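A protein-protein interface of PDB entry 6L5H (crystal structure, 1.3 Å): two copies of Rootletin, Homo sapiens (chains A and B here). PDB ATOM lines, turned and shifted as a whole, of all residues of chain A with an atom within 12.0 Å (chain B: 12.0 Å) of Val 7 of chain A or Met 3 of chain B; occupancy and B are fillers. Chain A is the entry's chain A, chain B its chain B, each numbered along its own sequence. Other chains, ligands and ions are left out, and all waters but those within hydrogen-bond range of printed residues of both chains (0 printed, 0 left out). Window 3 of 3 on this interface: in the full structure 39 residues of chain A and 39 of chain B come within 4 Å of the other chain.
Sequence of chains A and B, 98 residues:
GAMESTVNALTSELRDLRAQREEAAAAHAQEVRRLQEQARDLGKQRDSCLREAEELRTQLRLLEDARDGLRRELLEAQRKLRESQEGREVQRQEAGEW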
ATOM      1  N   MET A   3       3.487  20.917   6.025  1.00  0.00           N
ATOM      2  CA  MET A   3       3.058  19.536   6.225  1.00  0.00           C
ATOM      3  C   MET A   3       2.391  19.320   7.580  1.00  0.00           C
ATOM      4  O   MET A   3       2.689  20.010   8.557  1.00  0.00           O
ATOM      5  CB  MET A   3       4.245  18.577   6.088  1.00  0.00           C
ATOM      6  CG  MET A   3       4.499  18.086   4.672  1.00  0.00           C
ATOM      7  SD  MET A   3       2.946  17.195   3.893  1.00  0.00           S
ATOM      8  CE  MET A   3       2.668  15.806   5.232  1.00  0.00           C
ATOM      9  N   GLU A   4       1.474  18.355   7.629  1.00  0.00           N
ATOM     10  CA  GLU A   4       0.913  17.934   8.905  1.00  0.00           C
ATOM     11  C   GLU A   4       1.898  17.081   9.693  1.00  0.00           C
ATOM     12  O   GLU A   4       1.859  17.078  10.929  1.00  0.00           O
ATOM     13  CB  GLU A   4      -0.394  17.174   8.674  1.00  0.00           C
ATOM     14  CG  GLU A   4      -0.369  16.271   7.451  1.00  0.00           C
ATOM     15  CD  GLU A   4      -1.758  15.913   6.960  1.00  0.00           C
ATOM     16  OE1 GLU A   4      -2.726  16.090   7.729  1.00  0.00           O
ATOM     17  OE2 GLU A   4      -1.882  15.461   5.802  1.00  0.00           O
ATOM     18  N   SER A   5       2.795  16.374   8.999  1.00  0.00           N
ATOM     19  CA  SER A   5       3.790  15.554   9.684  1.00  0.00           C
ATOM     20  C   SER A   5       4.755  16.413  10.491  1.00  0.00           C
ATOM     21  O   SER A   5       5.158  16.028  11.595  1.00  0.00           O
ATOM     22  CB  SER A   5       4.554  14.697   8.674  1.00  0.00           C
ATOM     23  OG  SER A   5       3.676  13.807   8.004  1.00  0.00           O
ATOM     24  N   THR A   6       5.137  17.579   9.966  1.00  0.00           N
ATOM     25  CA  THR A   6       6.069  18.419  10.711  1.00  0.00           C
ATOM     26  C   THR A   6       5.380  19.135  11.868  1.00  0.00           C
ATOM     27  O   THR A   6       5.966  19.266  12.947  1.00  0.00           O
ATOM     28  CB  THR A   6       6.757  19.426   9.784  1.00  0.00           C
ATOM     29  OG1 THR A   6       7.570  20.312  10.566  1.00  0.00           O
ATOM     30  CG2 THR A   6       5.742  20.233   9.002  1.00  0.00           C
ATOM     31  N   VAL A   7       4.136  19.585  11.679  1.00  0.00           N
ATOM     32  CA  VAL A   7       3.419  20.242  12.769  1.00  0.00           C
ATOM     33  C   VAL A   7       3.133  19.251  13.893  1.00  0.00           C
ATOM     34  O   VAL A   7       3.341  19.554  15.083  1.00  0.00           O
ATOM     35  CB  VAL A   7       2.128  20.901  12.245  1.00  0.00           C
ATOM     36  CG1 VAL A   7       1.285  21.431  13.402  1.00  0.00           C
ATOM     37  CG2 VAL A   7       2.460  22.024  11.262  1.00  0.00           C
ATOM     38  N   ASN A   8       2.672  18.049  13.544  1.00  0.00           N
ATOM     39  CA  ASN A   8       2.344  17.068  14.574  1.00  0.00           C
ATOM     40  C   ASN A   8       3.595  16.530  15.263  1.00  0.00           C
ATOM     41  O   ASN A   8       3.555  16.235  16.465  1.00  0.00           O
ATOM     42  CB  ASN A   8       1.515  15.933  13.968  1.00  0.00           C
ATOM     43  CG  ASN A   8       0.123  16.388  13.550  1.00  0.00           C
ATOM     44  OD1 ASN A   8      -0.443  17.318  14.135  1.00  0.00           O
ATOM     45  ND2 ASN A   8      -0.437  15.733  12.540  1.00  0.00           N
ATOM     46  N   ALA A   9       4.713  16.416  14.539  1.00  0.00           N
ATOM     47  CA  ALA A   9       5.966  16.045  15.200  1.00  0.00           C
ATOM     48  C   ALA A   9       6.375  17.085  16.237  1.00  0.00           C
ATOM     49  O   ALA A   9       6.832  16.735  17.335  1.00  0.00           O
ATOM     50  CB  ALA A   9       7.087  15.870  14.178  1.00  0.00           C
ATOM     51  N   LEU A  10       6.231  18.370  15.901  1.00  0.00           N
ATOM     52  CA  LEU A  10       6.607  19.414  16.850  1.00  0.00           C
ATOM     53  C   LEU A  10       5.655  19.444  18.039  1.00  0.00           C
ATOM     54  O   LEU A  10       6.087  19.654  19.177  1.00  0.00           O
ATOM     55  CB  LEU A  10       6.642  20.780  16.159  1.00  0.00           C
ATOM     56  CG  LEU A  10       7.694  20.979  15.059  1.00  0.00           C
ATOM     57  CD1 LEU A  10       7.566  22.346  14.401  1.00  0.00           C
ATOM     58  CD2 LEU A  10       9.109  20.771  15.574  1.00  0.00           C
ATOM     59  N   THR A  11       4.356  19.242  17.799  1.00  0.00           N
ATOM     60  CA  THR A  11       3.410  19.177  18.910  1.00  0.00           C
ATOM     61  C   THR A  11       3.737  18.019  19.854  1.00  0.00           C
ATOM     62  O   THR A  11       3.687  18.171  21.085  1.00  0.00           O
ATOM     63  CB  THR A  11       1.985  19.064  18.359  1.00  0.00           C
ATOM     64  OG1 THR A  11       1.702  20.208  17.541  1.00  0.00           O
ATOM     65  CG2 THR A  11       0.976  19.006  19.490  1.00  0.00           C
ATOM     66  N   SER A  12       4.107  16.859  19.298  1.00  0.00           N
ATOM     67  CA  SER A  12       4.481  15.720  20.136  1.00  0.00           C
ATOM     68  C   SER A  12       5.744  16.017  20.946  1.00  0.00           C
ATOM     69  O   SER A  12       5.822  15.733  22.156  1.00  0.00           O
ATOM     70  CB  SER A  12       4.682  14.492  19.251  1.00  0.00           C
ATOM     71  OG  SER A  12       5.287  13.439  19.960  1.00  0.00           O
ATOM     72  N   GLU A  13       6.757  16.577  20.281  1.00  0.00           N
ATOM     73  CA  GLU A  13       7.997  16.911  20.973  1.00  0.00           C
ATOM     74  C   GLU A  13       7.756  17.933  22.080  1.00  0.00           C
ATOM     75  O   GLU A  13       8.386  17.880  23.150  1.00  0.00           O
ATOM     76  CB  GLU A  13       9.018  17.441  19.968  1.00  0.00           C
ATOM     77  CG  GLU A  13      10.399  17.586  20.561  1.00  0.00           C
ATOM     78  CD  GLU A  13      11.432  17.955  19.524  1.00  0.00           C
ATOM     79  OE1 GLU A  13      11.062  18.157  18.347  1.00  0.00           O
ATOM     80  OE2 GLU A  13      12.615  18.049  19.895  1.00  0.00           O
ATOM     81  N   LEU A  14       6.841  18.872  21.835  1.00  0.00           N
ATOM     82  CA  LEU A  14       6.515  19.895  22.820  1.00  0.00           C
ATOM     83  C   LEU A  14       5.872  19.287  24.052  1.00  0.00           C
ATOM     84  O   LEU A  14       6.213  19.656  25.181  1.00  0.00           O
ATOM     85  CB  LEU A  14       5.582  20.935  22.209  1.00  0.00           C
ATOM     86  CG  LEU A  14       6.258  22.157  21.609  1.00  0.00           C
ATOM     87  CD1 LEU A  14       5.233  22.997  20.887  1.00  0.00           C
ATOM     88  CD2 LEU A  14       6.935  22.966  22.701  1.00  0.00           C
ATOM     89  N   ARG A  15       4.922  18.368  23.863  1.00  0.00           N
ATOM     90  CA  ARG A  15       4.321  17.737  25.037  1.00  0.00           C
ATOM     91  C   ARG A  15       5.372  16.996  25.848  1.00  0.00           C
ATOM     92  O   ARG A  15       5.372  17.059  27.091  1.00  0.00           O
ATOM     93  CB  ARG A  15       3.187  16.793  24.637  1.00  0.00           C
ATOM     94  CG  ARG A  15       1.897  17.514  24.264  1.00  0.00           C
ATOM     95  CD  ARG A  15       0.670  16.606  24.352  1.00  0.00           C
ATOM     96  NE  ARG A  15      -0.523  17.327  23.934  1.00  0.00           N
ATOM     97  CZ  ARG A  15      -0.917  17.400  22.667  1.00  0.00           C
ATOM     98  NH1 ARG A  15      -0.207  16.787  21.732  1.00  0.00           N
ATOM     99  NH2 ARG A  15      -2.013  18.074  22.331  1.00  0.00           N
ATOM    100  N   ASP A  16       6.300  16.314  25.161  1.00  0.00           N
ATOM    101  CA  ASP A  16       7.355  15.593  25.874  1.00  0.00           C
ATOM    102  C   ASP A  16       8.268  16.550  26.643  1.00  0.00           C
ATOM    103  O   ASP A  16       8.613  16.303  27.818  1.00  0.00           O
ATOM    104  CB  ASP A  16       8.158  14.749  24.886  1.00  0.00           C
ATOM    105  CG  ASP A  16       9.142  13.835  25.557  1.00  0.00           C
ATOM    106  OD1 ASP A  16       8.723  12.998  26.386  1.00  0.00           O
ATOM    107  OD2 ASP A  16      10.339  13.940  25.231  1.00  0.00           O
ATOM    108  N   ARG A  18       7.628  19.607  27.760  1.00  0.00           N
ATOM    109  CA  ARG A  18       6.962  20.207  28.919  1.00  0.00           C
ATOM    110  C   ARG A  18       6.881  19.218  30.076  1.00  0.00           C
ATOM    111  O   ARG A  18       7.073  19.595  31.251  1.00  0.00           O
ATOM    112  CB  ARG A  18       5.562  20.700  28.552  1.00  0.00           C
ATOM    113  CG  ARG A  18       5.543  21.943  27.670  1.00  0.00           C
ATOM    114  CD  ARG A  18       4.150  22.578  27.607  1.00  0.00           C
ATOM    115  NE  ARG A  18       3.096  21.611  27.311  1.00  0.00           N
ATOM    116  CZ  ARG A  18       2.713  21.278  26.080  1.00  0.00           C
ATOM    117  NH1 ARG A  18       3.292  21.830  25.020  1.00  0.00           N
ATOM    118  NH2 ARG A  18       1.740  20.393  25.901  1.00  0.00           N
ATOM    119  N   MET B   3       1.424  27.345   6.189  1.00  0.00           N
ATOM    120  CA  MET B   3       1.609  26.724   7.500  1.00  0.00           C
ATOM    121  C   MET B   3       2.897  27.181   8.181  1.00  0.00           C
ATOM    122  O   MET B   3       3.208  26.743   9.287  1.00  0.00           O
ATOM    123  CB  MET B   3       1.609  25.202   7.374  1.00  0.00           C
ATOM    124  CG  MET B   3       0.250  24.609   7.051  1.00  0.00           C
ATOM    125  SD  MET B   3      -1.086  25.110   8.374  1.00  0.00           S
ATOM    126  CE  MET B   3      -0.203  24.412   9.966  1.00  0.00           C
ATOM    127  N   GLU B   4       3.638  28.067   7.509  1.00  0.00           N
ATOM    128  CA  GLU B   4       4.945  28.475   8.014  1.00  0.00           C
ATOM    129  C   GLU B   4       4.838  29.110   9.394  1.00  0.00           C
ATOM    130  O   GLU B   4       5.664  28.836  10.277  1.00  0.00           O
ATOM    131  CB  GLU B   4       5.603  29.440   7.024  1.00  0.00           C
ATOM    132  CG  GLU B   4       4.675  30.530   6.505  1.00  0.00           C
ATOM    133  CD  GLU B   4       5.345  31.433   5.481  1.00  0.00           C
ATOM    134  OE1 GLU B   4       6.593  31.515   5.498  1.00  0.00           O
ATOM    135  OE2 GLU B   4       4.625  32.052   4.659  1.00  0.00           O
ATOM    136  N   SER B   5       3.825  29.955   9.604  1.00  0.00           N
ATOM    137  CA  SER B   5       3.731  30.678  10.868  1.00  0.00           C
ATOM    138  C   SER B   5       3.455  29.728  12.030  1.00  0.00           C
ATOM    139  O   SER B   5       4.000  29.908  13.126  1.00  0.00           O
ATOM    140  CB  SER B   5       2.662  31.769  10.769  1.00  0.00           C
ATOM    141  OG  SER B   5       1.365  31.217  10.708  1.00  0.00           O
ATOM    142  N   THR B   6       2.644  28.690  11.804  1.00  0.00           N
ATOM    143  CA  THR B   6       2.375  27.719  12.865  1.00  0.00           C
ATOM    144  C   THR B   6       3.623  26.905  13.201  1.00  0.00           C
ATOM    145  O   THR B   6       3.943  26.689  14.379  1.00  0.00           O
ATOM    146  CB  THR B   6       1.225  26.795  12.457  1.00  0.00           C
ATOM    147  OG1 THR B   6       0.079  27.580  12.103  1.00  0.00           O
ATOM    148  CG2 THR B   6       0.852  25.870  13.614  1.00  0.00           C
ATOM    149  N   VAL B   7       4.331  26.427  12.168  1.00  0.00           N
ATOM    150  CA  VAL B   7       5.589  25.716  12.389  1.00  0.00           C
ATOM    151  C   VAL B   7       6.582  26.596  13.142  1.00  0.00           C
ATOM    152  O   VAL B   7       7.255  26.138  14.075  1.00  0.00           O
ATOM    153  CB  VAL B   7       6.168  25.236  11.046  1.00  0.00           C
ATOM    154  CG1 VAL B   7       7.546  24.619  11.248  1.00  0.00           C
ATOM    155  CG2 VAL B   7       5.221  24.244  10.376  1.00  0.00           C
ATOM    156  N   ASN B   8       6.700  27.863  12.739  1.00  0.00           N
ATOM    157  CA  ASN B   8       7.622  28.774  13.410  1.00  0.00           C
ATOM    158  C   ASN B   8       7.244  28.965  14.867  1.00  0.00           C
ATOM    159  O   ASN B   8       8.120  29.013  15.734  1.00  0.00           O
ATOM    160  CB  ASN B   8       7.645  30.127  12.709  1.00  0.00           C
ATOM    161  CG  ASN B   8       8.281  30.061  11.354  1.00  0.00           C
ATOM    162  OD1 ASN B   8       8.936  29.077  11.011  1.00  0.00           O
ATOM    163  ND2 ASN B   8       8.100  31.112  10.566  1.00  0.00           N
ATOM    164  N   ALA B   9       5.942  29.073  15.152  1.00  0.00           N
ATOM    165  CA  ALA B   9       5.503  29.270  16.530  1.00  0.00           C
ATOM    166  C   ALA B   9       5.851  28.066  17.398  1.00  0.00           C
ATOM    167  O   ALA B   9       6.332  28.221  18.535  1.00  0.00           O
ATOM    168  CB  ALA B   9       3.997  29.543  16.554  1.00  0.00           C
ATOM    169  N   LEU B  10       5.620  26.857  16.878  1.00  0.00           N
ATOM    170  CA  LEU B  10       5.948  25.655  17.643  1.00  0.00           C
ATOM    171  C   LEU B  10       7.451  25.517  17.837  1.00  0.00           C
ATOM    172  O   LEU B  10       7.908  25.151  18.924  1.00  0.00           O
ATOM    173  CB  LEU B  10       5.385  24.407  16.956  1.00  0.00           C
ATOM    174  CG  LEU B  10       3.861  24.313  16.884  1.00  0.00           C
ATOM    175  CD1 LEU B  10       3.435  23.144  16.013  1.00  0.00           C
ATOM    176  CD2 LEU B  10       3.239  24.188  18.256  1.00  0.00           C
ATOM    177  N   THR B  11       8.240  25.805  16.797  1.00  0.00           N
ATOM    178  CA  THR B  11       9.695  25.749  16.938  1.00  0.00           C
ATOM    179  C   THR B  11      10.187  26.761  17.962  1.00  0.00           C
ATOM    180  O   THR B  11      11.099  26.470  18.742  1.00  0.00           O
ATOM    181  CB  THR B  11      10.355  25.997  15.582  1.00  0.00           C
ATOM    182  OG1 THR B  11       9.974  24.948  14.695  1.00  0.00           O
ATOM    183  CG2 THR B  11      11.873  26.008  15.705  1.00  0.00           C
ATOM    184  N   SER B  12       9.595  27.955  17.963  1.00  0.00           N
ATOM    185  CA  SER B  12       9.933  28.982  18.947  1.00  0.00           C
ATOM    186  C   SER B  12       9.693  28.478  20.359  1.00  0.00           C
ATOM    187  O   SER B  12      10.545  28.636  21.241  1.00  0.00           O
ATOM    188  CB  SER B  12       9.092  30.236  18.676  1.00  0.00           C
ATOM    189  OG  SER B  12       9.218  31.201  19.711  1.00  0.00           O
ATOM    190  N   GLU B  13       8.535  27.848  20.582  1.00  0.00           N
ATOM    191  CA  GLU B  13       8.232  27.293  21.899  1.00  0.00           C
ATOM    192  C   GLU B  13       9.222  26.190  22.284  1.00  0.00           C
ATOM    193  O   GLU B  13       9.689  26.122  23.434  1.00  0.00           O
ATOM    194  CB  GLU B  13       6.794  26.780  21.893  1.00  0.00           C
ATOM    195  CG  GLU B  13       6.204  26.476  23.233  1.00  0.00           C
ATOM    196  CD  GLU B  13       4.708  26.253  23.139  1.00  0.00           C
ATOM    197  OE1 GLU B  13       4.147  26.367  22.017  1.00  0.00           O
ATOM    198  OE2 GLU B  13       4.096  25.953  24.181  1.00  0.00           O
ATOM    199  N   LEU B  14       9.568  25.316  21.333  1.00  0.00           N
ATOM    200  CA  LEU B  14      10.531  24.259  21.628  1.00  0.00           C
ATOM    201  C   LEU B  14      11.888  24.833  22.011  1.00  0.00           C
ATOM    202  O   LEU B  14      12.528  24.365  22.959  1.00  0.00           O
ATOM    203  CB  LEU B  14      10.675  23.319  20.430  1.00  0.00           C
ATOM    204  CG  LEU B  14       9.556  22.296  20.233  1.00  0.00           C
ATOM    205  CD1 LEU B  14       9.600  21.771  18.827  1.00  0.00           C
ATOM    206  CD2 LEU B  14       9.706  21.146  21.216  1.00  0.00           C
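Val 7 of chain A touches just these residues of chain B: Met 3 (3.8 Å), Val 7 (3.7 Å) and Leu 10 (3.7 Å).
Of the printed residues of chain A, Met 3 of chain B touches Val 7.
No residue of chain B comes within 4 Å of Ser 5 of chain A.
No residue of chain B comes within 4 Å of Thr 6 of chain A.
No residue of chain B comes within 4 Å of Asn 8 of chain A.
No residue of chain B comes within 4 Å of Ala 9 of chain A.
Leu 10 of chain A touches just these residues of chain B: Val 7, Leu 10, Thr 11 and Leu 14.
Glu 4 of chain B touches none of the printed residues of chain A.
No residue of chain A comes within 4 Å of Ser 5 of chain B.
Thr 6 of chain B touches none of the printed residues of chain A.
Of chain A, only Val 7 (3.7 Å) and Leu 10 (3.8 Å) come within 4 Å of Val 7 of chain B.
Printed residues of chain A within 4 Å of Glu 13 of chain B: Leu 14.
Of the printed residues of chain B, Glu 13 of chain A touches Leu 14.
Printed residues of chain A within 4 Å of Leu 10 of chain B: Val 7, Leu 10, Thr 11 and Leu 14.
Met 3 of chain A touches none of the printed residues of chain B.
Asn 8 of chain B touches none of the printed residues of chain A.
The nearest residue of chain A that does not touch Met 3 of chain B is Met 3 of chain A (4.9 Å).
The nearest printed residue of chain B that does not touch Glu 13 of chain A is Leu 10 of chain B (7.7 Å).
Met 3 of chain B touches Val 7 of chain A.
Val 7 of chain B touches Leu 10 of chain A (O to CD1, 3.8 Å).
Leu 10 of chain B touches Leu 10 of chain A.
Leu 10 of chain A touches Thr 11 of chain B (CD1 to OG1, 3.6 Å).
Leu 10 of chain A touches Leu 14 of chain B (CD2 to CD1, 3.4 Å).
Leu 10 of chain B touches Thr 11 of chain A (CD1 to OG1, 3.7 Å).
Glu 13 of chain A touches Leu 14 of chain B (CG to CD2, 3.7 Å).
Leu 14 of chain A touches Leu 10 of chain B.
Leu 14 of chain A touches Glu 13 of chain B.
Leu 14 of chain B touches Leu 14 of chain A.
Val 7 of chain B touches its own counterpart, Val 7 of chain A.
Val 7 of chain A touches Leu 10 of chain B, and with the chains exchanged Leu 10 of chain A touches Val 7 of chain B.
Leu 10 of chain A touches Leu 14 of chain B, and with the chains exchanged Leu 14 of chain A touches Leu 10 of chain B.
Glu 13 of chain A touches Leu 14 of chain B, and with the chains exchanged Leu 14 of chain A touches Glu 13 of chain B.
Of the 12 printed residues of chain B, 6 touch a printed residue of chain A.
Hydrophobic or aromatic side chains of chain B that line the printed part of chain A: Met 3, Val 7, Leu 10 and Leu 14.
Hydrophobic or aromatic side chains of chain A that line the printed part of chain B: Val 7, Leu 10 and Leu 14.
OG1 of Thr 11 of chain B sits at hydrogen-bond distance from O of Val 7 of chain B (3.0 Å).
OG1 of Thr 11 of chain A is in hydrogen-bond range of O of Val 7 of chain A (3.0 Å).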
